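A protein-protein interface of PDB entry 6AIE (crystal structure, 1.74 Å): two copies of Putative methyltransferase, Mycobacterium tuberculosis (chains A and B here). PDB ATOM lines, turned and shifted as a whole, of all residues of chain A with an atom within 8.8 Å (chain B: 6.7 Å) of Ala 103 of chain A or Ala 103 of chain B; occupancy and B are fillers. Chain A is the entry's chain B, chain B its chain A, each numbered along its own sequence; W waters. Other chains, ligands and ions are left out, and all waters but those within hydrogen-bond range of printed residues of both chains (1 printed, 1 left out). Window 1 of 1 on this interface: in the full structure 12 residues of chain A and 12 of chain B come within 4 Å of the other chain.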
ATOM      1  N   LEU A  51      21.610  10.966   0.941  1.00  0.00           N
ATOM      2  CA  LEU A  51      20.197  10.760   0.615  1.00  0.00           C
ATOM      3  C   LEU A  51      19.567   9.760   1.549  1.00  0.00           C
ATOM      4  O   LEU A  51      20.178   8.778   1.868  1.00  0.00           O
ATOM      5  CB  LEU A  51      20.027  10.267  -0.813  1.00  0.00           C
ATOM      6  CG  LEU A  51      20.549  11.132  -1.944  1.00  0.00           C
ATOM      7  CD1 LEU A  51      20.438  10.323  -3.256  1.00  0.00           C
ATOM      8  CD2 LEU A  51      19.759  12.437  -1.977  1.00  0.00           C
ATOM      9  N   TYR A  52      18.323  10.029   1.936  1.00  0.00           N
ATOM     10  CA  TYR A  52      17.597   9.274   2.976  1.00  0.00           C
ATOM     11  C   TYR A  52      18.483   9.301   4.247  1.00  0.00           C
ATOM     12  O   TYR A  52      18.741   8.280   4.855  1.00  0.00           O
ATOM     13  CB  TYR A  52      17.298   7.838   2.530  1.00  0.00           C
ATOM     14  CG  TYR A  52      16.709   7.682   1.167  1.00  0.00           C
ATOM     15  CD1 TYR A  52      15.336   7.721   0.999  1.00  0.00           C
ATOM     16  CD2 TYR A  52      17.493   7.381   0.088  1.00  0.00           C
ATOM     17  CE1 TYR A  52      14.770   7.555  -0.223  1.00  0.00           C
ATOM     18  CE2 TYR A  52      16.915   7.244  -1.159  1.00  0.00           C
ATOM     19  CZ  TYR A  52      15.546   7.294  -1.281  1.00  0.00           C
ATOM     20  OH  TYR A  52      14.926   7.144  -2.485  1.00  0.00           O
ATOM     21  N   VAL A  73      19.528  15.008   2.682  1.00  0.00           N
ATOM     22  CA  VAL A  73      18.189  15.032   2.209  1.00  0.00           C
ATOM     23  C   VAL A  73      17.435  13.930   2.982  1.00  0.00           C
ATOM     24  O   VAL A  73      17.869  12.769   2.964  1.00  0.00           O
ATOM     25  CB  VAL A  73      18.102  14.815   0.687  1.00  0.00           C
ATOM     26  CG1 VAL A  73      16.696  15.066   0.221  1.00  0.00           C
ATOM     27  CG2 VAL A  73      19.181  15.670  -0.059  1.00  0.00           C
ATOM     28  N   GLU A  74      16.329  14.304   3.598  1.00  0.00           N
ATOM     29  CA  GLU A  74      15.535  13.436   4.464  1.00  0.00           C
ATOM     30  C   GLU A  74      14.088  13.866   4.492  1.00  0.00           C
ATOM     31  O   GLU A  74      13.808  15.020   4.699  1.00  0.00           O
ATOM     32  CB  GLU A  74      16.123  13.451   5.894  1.00  0.00           C
ATOM     33  CG  GLU A  74      15.318  12.713   6.962  1.00  0.00           C
ATOM     34  CD  GLU A  74      15.016  11.258   6.606  1.00  0.00           C
ATOM     35  OE1 GLU A  74      15.932  10.504   6.221  1.00  0.00           O
ATOM     36  OE2 GLU A  74      13.832  10.869   6.711  1.00  0.00           O
ATOM     37  N   SER A  75      13.158  12.949   4.306  1.00  0.00           N
ATOM     38  CA  SER A  75      11.731  13.307   4.241  1.00  0.00           C
ATOM     39  C   SER A  75      11.031  13.363   5.622  1.00  0.00           C
ATOM     40  O   SER A  75      10.145  14.160   5.823  1.00  0.00           O
ATOM     41  CB  SER A  75      10.953  12.383   3.294  1.00  0.00           C
ATOM     42  OG  SER A  75      10.975  11.098   3.815  1.00  0.00           O
ATOM     43  N   GLY A 100      12.497  16.991   2.659  1.00  0.00           N
ATOM     44  CA  GLY A 100      11.591  16.818   1.523  1.00  0.00           C
ATOM     45  C   GLY A 100      11.654  15.390   0.998  1.00  0.00           C
ATOM     46  O   GLY A 100      12.534  14.573   1.374  1.00  0.00           O
ATOM     47  N   ALA A 101      10.739  15.089   0.071  1.00  0.00           N
ATOM     48  CA  ALA A 101      10.683  13.775  -0.499  1.00  0.00           C
ATOM     49  C   ALA A 101      11.941  13.560  -1.354  1.00  0.00           C
ATOM     50  O   ALA A 101      12.228  14.332  -2.284  1.00  0.00           O
ATOM     51  CB  ALA A 101       9.406  13.584  -1.324  1.00  0.00           C
ATOM     52  N   VAL A 102      12.717  12.539  -1.016  1.00  0.00           N
ATOM     53  CA  VAL A 102      14.042  12.411  -1.569  1.00  0.00           C
ATOM     54  C   VAL A 102      14.063  12.280  -3.107  1.00  0.00           C
ATOM     55  O   VAL A 102      14.891  12.893  -3.810  1.00  0.00           O
ATOM     56  CB  VAL A 102      14.765  11.221  -0.930  1.00  0.00           C
ATOM     57  CG1 VAL A 102      16.114  10.925  -1.614  1.00  0.00           C
ATOM     58  CG2 VAL A 102      15.016  11.494   0.566  1.00  0.00           C
ATOM     59  N   ALA A 103      13.214  11.414  -3.647  1.00  0.00           N
ATOM     60  CA  ALA A 103      13.181  11.262  -5.106  1.00  0.00           C
ATOM     61  C   ALA A 103      12.710  12.517  -5.842  1.00  0.00           C
ATOM     62  O   ALA A 103      13.167  12.830  -6.981  1.00  0.00           O
ATOM     63  CB  ALA A 103      12.332  10.061  -5.488  1.00  0.00           C
ATOM     64  N   ALA A 104      11.825  13.268  -5.217  1.00  0.00           N
ATOM     65  CA  ALA A 104      11.383  14.501  -5.799  1.00  0.00           C
ATOM     66  C   ALA A 104      12.508  15.548  -5.809  1.00  0.00           C
ATOM     67  O   ALA A 104      12.700  16.234  -6.784  1.00  0.00           O
ATOM     68  CB  ALA A 104      10.206  15.025  -5.029  1.00  0.00           C
ATOM     69  N   VAL A 105      13.298  15.616  -4.755  1.00  0.00           N
ATOM     70  CA  VAL A 105      14.514  16.463  -4.720  1.00  0.00           C
ATOM     71  C   VAL A 105      15.470  16.060  -5.813  1.00  0.00           C
ATOM     72  O   VAL A 105      15.941  16.894  -6.613  1.00  0.00           O
ATOM     73  CB  VAL A 105      15.180  16.374  -3.326  1.00  0.00           C
ATOM     74  CG1 VAL A 105      16.554  17.050  -3.326  1.00  0.00           C
ATOM     75  CG2 VAL A 105      14.277  17.001  -2.286  1.00  0.00           C
ATOM     76  N   VAL A 106      15.719  14.765  -5.899  1.00  0.00           N
ATOM     77  CA  VAL A 106      16.595  14.261  -6.922  1.00  0.00           C
ATOM     78  C   VAL A 106      16.076  14.571  -8.325  1.00  0.00           C
ATOM     79  O   VAL A 106      16.833  14.991  -9.220  1.00  0.00           O
ATOM     80  CB  VAL A 106      16.925  12.782  -6.756  1.00  0.00           C
ATOM     81  CG1 VAL A 106      17.812  12.295  -7.908  1.00  0.00           C
ATOM     82  CG2 VAL A 106      17.680  12.517  -5.451  1.00  0.00           C
ATOM     83  N   ALA A 107      14.786  14.413  -8.501  1.00  0.00           N
ATOM     84  CA  ALA A 107      14.137  14.743  -9.816  1.00  0.00           C
ATOM     85  C   ALA A 107      14.396  16.178 -10.325  1.00  0.00           C
ATOM     86  O   ALA A 107      14.674  16.403 -11.528  1.00  0.00           O
ATOM     87  CB  ALA A 107      12.659  14.514  -9.700  1.00  0.00           C
ATOM     88  N   ALA A 108      14.301  17.129  -9.391  1.00  0.00           N
ATOM     89  CA  ALA A 108      14.376  18.546  -9.705  1.00  0.00           C
ATOM     90  C   ALA A 108      15.826  18.948  -9.967  1.00  0.00           C
ATOM     91  O   ALA A 108      16.068  19.965 -10.614  1.00  0.00           O
ATOM     92  CB  ALA A 108      13.771  19.387  -8.580  1.00  0.00           C
ATOM     93  N   GLY A 109      16.795  18.190  -9.460  1.00  0.00           N
ATOM     94  CA  GLY A 109      18.168  18.371  -9.918  1.00  0.00           C
ATOM     95  C   GLY A 109      18.925  19.534  -9.250  1.00  0.00           C
ATOM     96  O   GLY A 109      18.494  20.089  -8.193  1.00  0.00           O
ATOM     97  N   VAL A 125      11.645   0.754   0.121  1.00  0.00           N
ATOM     98  CA  VAL A 125      11.953   1.363  -1.182  1.00  0.00           C
ATOM     99  C   VAL A 125      12.511   0.272  -2.061  1.00  0.00           C
ATOM    100  O   VAL A 125      13.525  -0.362  -1.719  1.00  0.00           O
ATOM    101  CB  VAL A 125      12.981   2.527  -1.083  1.00  0.00           C
ATOM    102  CG1 VAL A 125      13.345   3.040  -2.472  1.00  0.00           C
ATOM    103  CG2 VAL A 125      12.459   3.679  -0.207  1.00  0.00           C
ATOM    104  N   ASP A 129      13.222   1.311  -7.968  1.00  0.00           N
ATOM    105  CA  ASP A 129      13.085   2.763  -7.706  1.00  0.00           C
ATOM    106  C   ASP A 129      14.409   3.388  -7.342  1.00  0.00           C
ATOM    107  O   ASP A 129      14.742   4.456  -7.852  1.00  0.00           O
ATOM    108  CB  ASP A 129      11.990   3.056  -6.677  1.00  0.00           C
ATOM    109  CG  ASP A 129      10.619   2.552  -7.152  1.00  0.00           C
ATOM    110  OD1 ASP A 129      10.240   2.800  -8.326  1.00  0.00           O
ATOM    111  OD2 ASP A 129       9.938   1.867  -6.372  1.00  0.00           O
ATOM    112  N   VAL A 130      15.234   2.678  -6.544  1.00  0.00           N
ATOM    113  CA  VAL A 130      16.632   3.122  -6.378  1.00  0.00           C
ATOM    114  C   VAL A 130      17.369   3.239  -7.734  1.00  0.00           C
ATOM    115  O   VAL A 130      18.140   4.197  -7.927  1.00  0.00           O
ATOM    116  CB  VAL A 130      17.396   2.242  -5.366  1.00  0.00           C
ATOM    117  CG1 VAL A 130      18.829   2.746  -5.120  1.00  0.00           C
ATOM    118  CG2 VAL A 130      16.629   2.142  -4.064  1.00  0.00           C
ATOM    119  N   ALA A 132      16.255   3.955 -10.640  1.00  0.00           N
ATOM    120  CA  ALA A 132      15.817   5.163 -11.321  1.00  0.00           C
ATOM    121  C   ALA A 132      16.452   6.438 -10.701  1.00  0.00           C
ATOM    122  O   ALA A 132      16.797   7.354 -11.405  1.00  0.00           O
ATOM    123  CB  ALA A 132      14.323   5.285 -11.277  1.00  0.00           C
ATOM    124  N   ILE A 133      16.633   6.436  -9.377  1.00  0.00           N
ATOM    125  CA  ILE A 133      17.397   7.467  -8.671  1.00  0.00           C
ATOM    126  C   ILE A 133      18.823   7.519  -9.161  1.00  0.00           C
ATOM    127  O   ILE A 133      19.386   8.614  -9.379  1.00  0.00           O
ATOM    128  CB  ILE A 133      17.306   7.285  -7.134  1.00  0.00           C
ATOM    129  CG1 ILE A 133      15.828   7.402  -6.645  1.00  0.00           C
ATOM    130  CG2 ILE A 133      18.189   8.262  -6.379  1.00  0.00           C
ATOM    131  CD1 ILE A 133      15.250   8.737  -6.858  1.00  0.00           C
ATOM    132  N   ALA A 136      18.895   9.205 -12.479  1.00  0.00           N
ATOM    133  CA  ALA A 136      18.618  10.594 -12.216  1.00  0.00           C
ATOM    134  C   ALA A 136      19.864  11.308 -11.707  1.00  0.00           C
ATOM    135  O   ALA A 136      20.132  12.442 -12.159  1.00  0.00           O
ATOM    136  CB  ALA A 136      17.417  10.779 -11.249  1.00  0.00           C
ATOM    137  N   LEU A 137      20.638  10.661 -10.825  1.00  0.00           N
ATOM    138  CA  LEU A 137      21.899  11.269 -10.317  1.00  0.00           C
ATOM    139  C   LEU A 137      22.873  11.639 -11.405  1.00  0.00           C
ATOM    140  O   LEU A 137      23.456  12.738 -11.365  1.00  0.00           O
ATOM    141  CB  LEU A 137      22.595  10.375  -9.265  1.00  0.00           C
ATOM    142  CG  LEU A 137      21.836  10.275  -7.937  1.00  0.00           C
ATOM    143  CD1 LEU A 137      22.320   9.105  -7.105  1.00  0.00           C
ATOM    144  CD2 LEU A 137      22.016  11.556  -7.108  1.00  0.00           C
ATOM    145  N   ASN A 140      20.895  14.726 -13.965  1.00  0.00           N
ATOM    146  CA  ASN A 140      20.196  15.888 -13.454  1.00  0.00           C
ATOM    147  C   ASN A 140      21.081  16.873 -12.696  1.00  0.00           C
ATOM    148  O   ASN A 140      20.544  17.748 -11.978  1.00  0.00           O
ATOM    149  CB  ASN A 140      19.064  15.445 -12.516  1.00  0.00           C
ATOM    150  CG  ASN A 140      17.980  14.676 -13.212  1.00  0.00           C
ATOM    151  OD1 ASN A 140      18.007  14.434 -14.428  1.00  0.00           O
ATOM    152  ND2 ASN A 140      16.992  14.254 -12.416  1.00  0.00           N
ATOM    153  N   TRP A 142      23.645  16.190 -10.425  1.00  0.00           N
ATOM    154  CA  TRP A 142      24.233  15.781  -9.139  1.00  0.00           C
ATOM    155  C   TRP A 142      25.663  15.240  -9.196  1.00  0.00           C
ATOM    156  O   TRP A 142      26.386  15.268  -8.193  1.00  0.00           O
ATOM    157  CB  TRP A 142      23.338  14.803  -8.395  1.00  0.00           C
ATOM    158  CG  TRP A 142      21.961  15.239  -8.225  1.00  0.00           C
ATOM    159  CD1 TRP A 142      20.897  14.879  -8.997  1.00  0.00           C
ATOM    160  CD2 TRP A 142      21.449  16.084  -7.215  1.00  0.00           C
ATOM    161  NE1 TRP A 142      19.761  15.459  -8.529  1.00  0.00           N
ATOM    162  CE2 TRP A 142      20.070  16.213  -7.439  1.00  0.00           C
ATOM    163  CE3 TRP A 142      22.016  16.734  -6.113  1.00  0.00           C
ATOM    164  CZ2 TRP A 142      19.244  16.966  -6.616  1.00  0.00           C
ATOM    165  CZ3 TRP A 142      21.213  17.490  -5.327  1.00  0.00           C
ATOM    166  CH2 TRP A 142      19.830  17.602  -5.565  1.00  0.00           C
ATOM    167  N   TYR B  52       0.523   9.473 -10.868  1.00  0.00           N
ATOM    168  CA  TYR B  52      -0.270   9.062  -9.692  1.00  0.00           C
ATOM    169  C   TYR B  52      -1.635   8.641 -10.217  1.00  0.00           C
ATOM    170  O   TYR B  52      -2.683   9.028  -9.662  1.00  0.00           O
ATOM    171  CB  TYR B  52      -0.448  10.187  -8.667  1.00  0.00           C
ATOM    172  CG  TYR B  52       0.822  10.857  -8.235  1.00  0.00           C
ATOM    173  CD1 TYR B  52       1.590  10.314  -7.201  1.00  0.00           C
ATOM    174  CD2 TYR B  52       1.222  12.054  -8.795  1.00  0.00           C
ATOM    175  CE1 TYR B  52       2.743  10.937  -6.779  1.00  0.00           C
ATOM    176  CE2 TYR B  52       2.391  12.658  -8.397  1.00  0.00           C
ATOM    177  CZ  TYR B  52       3.126  12.117  -7.360  1.00  0.00           C
ATOM    178  OH  TYR B  52       4.318  12.684  -6.913  1.00  0.00           O
ATOM    179  N   VAL B  73       1.454   6.329 -14.831  1.00  0.00           N
ATOM    180  CA  VAL B  73       2.477   6.026 -13.877  1.00  0.00           C
ATOM    181  C   VAL B  73       1.767   5.903 -12.531  1.00  0.00           C
ATOM    182  O   VAL B  73       1.066   6.848 -12.124  1.00  0.00           O
ATOM    183  CB  VAL B  73       3.606   7.081 -13.856  1.00  0.00           C
ATOM    184  CG1 VAL B  73       4.715   6.634 -12.917  1.00  0.00           C
ATOM    185  CG2 VAL B  73       4.158   7.350 -15.267  1.00  0.00           C
ATOM    186  N   GLY B 100       5.660   2.067 -10.684  1.00  0.00           N
ATOM    187  CA  GLY B 100       6.829   2.443  -9.963  1.00  0.00           C
ATOM    188  C   GLY B 100       6.552   3.710  -9.187  1.00  0.00           C
ATOM    189  O   GLY B 100       5.461   4.327  -9.303  1.00  0.00           O
ATOM    190  N   ALA B 101       7.570   4.113  -8.413  1.00  0.00           N
ATOM    191  CA  ALA B 101       7.482   5.300  -7.596  1.00  0.00           C
ATOM    192  C   ALA B 101       7.541   6.504  -8.522  1.00  0.00           C
ATOM    193  O   ALA B 101       8.515   6.705  -9.286  1.00  0.00           O
ATOM    194  CB  ALA B 101       8.601   5.333  -6.567  1.00  0.00           C
ATOM    195  N   VAL B 102       6.500   7.302  -8.441  1.00  0.00           N
ATOM    196  CA  VAL B 102       6.220   8.298  -9.424  1.00  0.00           C
ATOM    197  C   VAL B 102       7.322   9.340  -9.473  1.00  0.00           C
ATOM    198  O   VAL B 102       7.772   9.732 -10.543  1.00  0.00           O
ATOM    199  CB  VAL B 102       4.854   8.966  -9.155  1.00  0.00           C
ATOM    200  CG1 VAL B 102       4.633  10.167 -10.047  1.00  0.00           C
ATOM    201  CG2 VAL B 102       3.684   7.952  -9.320  1.00  0.00           C
ATOM    202  N   ALA B 103       7.752   9.837  -8.327  1.00  0.00           N
ATOM    203  CA  ALA B 103       8.805  10.841  -8.361  1.00  0.00           C
ATOM    204  C   ALA B 103      10.118  10.289  -8.898  1.00  0.00           C
ATOM    205  O   ALA B 103      10.924  11.022  -9.524  1.00  0.00           O
ATOM    206  CB  ALA B 103       9.014  11.432  -6.986  1.00  0.00           C
ATOM    207  N   ALA B 104      10.367   9.009  -8.633  1.00  0.00           N
ATOM    208  CA  ALA B 104      11.586   8.381  -9.083  1.00  0.00           C
ATOM    209  C   ALA B 104      11.549   8.219 -10.626  1.00  0.00           C
ATOM    210  O   ALA B 104      12.515   8.491 -11.334  1.00  0.00           O
ATOM    211  CB  ALA B 104      11.752   7.049  -8.428  1.00  0.00           C
ATOM    212  N   VAL B 105      10.406   7.818 -11.152  1.00  0.00           N
ATOM    213  CA  VAL B 105      10.184   7.768 -12.617  1.00  0.00           C
ATOM    214  C   VAL B 105      10.433   9.135 -13.234  1.00  0.00           C
ATOM    215  O   VAL B 105      11.097   9.276 -14.274  1.00  0.00           O
ATOM    216  CB  VAL B 105       8.723   7.317 -12.928  1.00  0.00           C
ATOM    217  CG1 VAL B 105       8.450   7.468 -14.399  1.00  0.00           C
ATOM    218  CG2 VAL B 105       8.533   5.873 -12.556  1.00  0.00           C
ATOM    219  N   VAL B 106       9.874  10.159 -12.602  1.00  0.00           N
ATOM    220  CA  VAL B 106       9.971  11.492 -13.146  1.00  0.00           C
ATOM    221  C   VAL B 106      11.425  11.953 -13.124  1.00  0.00           C
ATOM    222  O   VAL B 106      11.959  12.537 -14.103  1.00  0.00           O
ATOM    223  CB  VAL B 106       9.084  12.453 -12.342  1.00  0.00           C
ATOM    224  CG1 VAL B 106       9.393  13.895 -12.738  1.00  0.00           C
ATOM    225  CG2 VAL B 106       7.614  12.157 -12.567  1.00  0.00           C
ATOM    226  N   ALA B 107      12.060  11.681 -11.992  1.00  0.00           N
ATOM    227  CA  ALA B 107      13.536  11.927 -11.813  1.00  0.00           C
ATOM    228  C   ALA B 107      14.455  11.348 -12.889  1.00  0.00           C
ATOM    229  O   ALA B 107      15.430  12.030 -13.387  1.00  0.00           O
ATOM    230  CB  ALA B 107      13.978  11.422 -10.447  1.00  0.00           C
ATOM    231  N   ALA B 108      14.151  10.117 -13.309  1.00  0.00           N
ATOM    232  CA  ALA B 108      14.990   9.462 -14.299  1.00  0.00           C
ATOM    233  C   ALA B 108      14.717  10.012 -15.724  1.00  0.00           C
ATOM    234  O   ALA B 108      15.526   9.813 -16.604  1.00  0.00           O
ATOM    235  CB  ALA B 108      14.762   7.950 -14.304  1.00  0.00           C
ATOM    236  N   ASP B 129       6.736  19.144  -2.535  1.00  0.00           N
ATOM    237  CA  ASP B 129       7.197  17.990  -3.301  1.00  0.00           C
ATOM    238  C   ASP B 129       6.602  17.923  -4.693  1.00  0.00           C
ATOM    239  O   ASP B 129       7.303  17.647  -5.632  1.00  0.00           O
ATOM    240  CB  ASP B 129       7.022  16.686  -2.522  1.00  0.00           C
ATOM    241  CG  ASP B 129       7.796  16.711  -1.183  1.00  0.00           C
ATOM    242  OD1 ASP B 129       9.005  17.067  -1.137  1.00  0.00           O
ATOM    243  OD2 ASP B 129       7.179  16.379  -0.171  1.00  0.00           O
ATOM    244  N   ILE B 133       8.505  18.135  -8.563  1.00  0.00           N
ATOM    245  CA  ILE B 133       8.040  17.353  -9.699  1.00  0.00           C
ATOM    246  C   ILE B 133       7.749  18.228 -10.912  1.00  0.00           C
ATOM    247  O   ILE B 133       8.097  17.869 -12.022  1.00  0.00           O
ATOM    248  CB  ILE B 133       6.775  16.522  -9.325  1.00  0.00           C
ATOM    249  CG1 ILE B 133       7.082  15.500  -8.210  1.00  0.00           C
ATOM    250  CG2 ILE B 133       6.274  15.724 -10.526  1.00  0.00           C
ATOM    251  CD1 ILE B 133       7.964  14.391  -8.582  1.00  0.00           C
ATOM    252  N   ALA B 136      10.996  19.264 -12.432  1.00  0.00           N
ATOM    253  CA  ALA B 136      11.560  18.097 -13.058  1.00  0.00           C
ATOM    254  C   ALA B 136      10.905  17.831 -14.389  1.00  0.00           C
ATOM    255  O   ALA B 136      11.617  17.433 -15.347  1.00  0.00           O
ATOM    256  CB  ALA B 136      11.418  16.888 -12.141  1.00  0.00           C
HETATM  257  O   HOH W   1       6.808   1.968  -6.308  1.00  0.00           O
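Printed residues of chain B within 4 Å of Ala 101 of chain A: Asp 129 (2.9 Å). Of chain B, only Ala 103, Ala 104 and Ala 107 come within 4 Å of Ala 103 of chain A. Of the printed residues of chain B, Ala 104 of chain A touches Ala 103 and Asp 129. Of the printed residues of chain B, Ala 108 of chain A touches Ala 136 (3.99 Å). Ile 133 of chain A touches none of the printed residues of chain B. Of the printed residues of chain A, Ala 107 of chain B touches Ala 103, Ala 107, Ala 136 and Asn 140. The nearest residue of chain A that does not touch Ala 103 of chain B is Ile 133 of chain A (5.6 Å). The nearest printed residue of chain B that does not touch Ala 101 of chain A is Ala 103 of chain B (6.1 Å).
Of the 24 printed residues of chain A, 10 touch a printed residue of chain B. Hydrophobic or aromatic side chains of chain A that line the printed part of chain B: Ala 101, Ala 103, Ala 104, Ala 107, Ala 132 and Ala 136. Printed residues of chain B that touch a printed residue of chain A: Gly 100, Ala 101, Ala 103, Ala 104, Ala 107, Ala 108, Asp 129 and Ala 136. Hydrophobic or aromatic side chains of chain B within 4 Å of the printed part of chain A: Ala 101, Ala 103, Ala 104, Ala 107, Ala 108 and Ala 136. Among the printed residues, 19 pairs touch across the chains. Among the printed residues, no Asp or Glu carboxylate lies within 4 Å of a Lys or Arg side-chain nitrogen of the other chain.
Asp 129 of chain B touches Gly 100 of chain A. O of Ala 103 of chain A touches O of Ala 103 of chain B (3.8 Å). Ala 103 of chain A touches Ala 107 of chain B. Ala 103 of chain B touches Ala 104 of chain A. CA of Ala 107 of chain A touches CB of Ala 107 of chain B, 3.4 Å away. Ala 107 of chain A touches Ala 136 of chain B (O to CB, 3.3 Å). Ala 108 of chain A touches Ala 136 of chain B (N to CB, 3.99 Å). OD1 of Asp 129 of chain A touches CA of Gly 100 of chain B, 3.8 Å away. Ala 104 of chain B touches Ala 132 of chain A. Ala 136 of chain A touches Ala 108 of chain B (CB to N, 3.9 Å).
ND2 of Asn 140 of chain A sits at hydrogen-bond distance from O of Ala 107 of chain B. N of Ala 101 of chain B lies within hydrogen-bond range of OD1 of Asp 129 of chain A (3.0 Å). The side-chain carboxylate of Asp 129 of chain B is in hydrogen-bond range of the backbone NH of Ala 101 of chain A (2.9 Å).
Water W1 lies within hydrogen-bond range of the backbone NH (N) of Ala 101 of chain B and the side-chain carboxylate (OD2) of Asp 129 of chain A.
Gly 100 of chain A touches Asp 129 of chain B, and with the chains exchanged Asp 129 of chain A touches Gly 100 of chain B. Ala 104 of chain A touches Asp 129 of chain B, and with the chains exchanged Asp 129 of chain A touches Ala 104 of chain B. Ala 107 of chain A touches Ala 136 of chain B, and with the chains exchanged Ala 136 of chain A touches Ala 107 of chain B. Ala 108 of chain A touches Ala 136 of chain B, and with the chains exchanged Ala 136 of chain A touches Ala 108 of chain B. Positions printed for both chains: 52, 73, 100, 101, 102, 103, 104, 105, 106, 107, 108, 129, 133 and 136. Of the 19 pairs that touch across the chains among the printed residues, 16 have their exchanged pair printed and touching as well.
O of Glu 74 of chain A is in hydrogen-bond range of N of Gly 100 of chain A (3.1 Å). The side-chain amide nitrogen (ND2) of Asn 140 of chain A lies within hydrogen-bond range of the backbone carbonyl oxygen (O) of Val 106 of chain A (3.3 Å). The backbone NH of Ser 75 of chain A lies close to the backbone carbonyl oxygen of Gly 100 of chain A (3.4 Å). O of Ala 107 of chain A is in hydrogen-bond range of ND2 of Asn 140 of chain A, at 3.3 Å.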
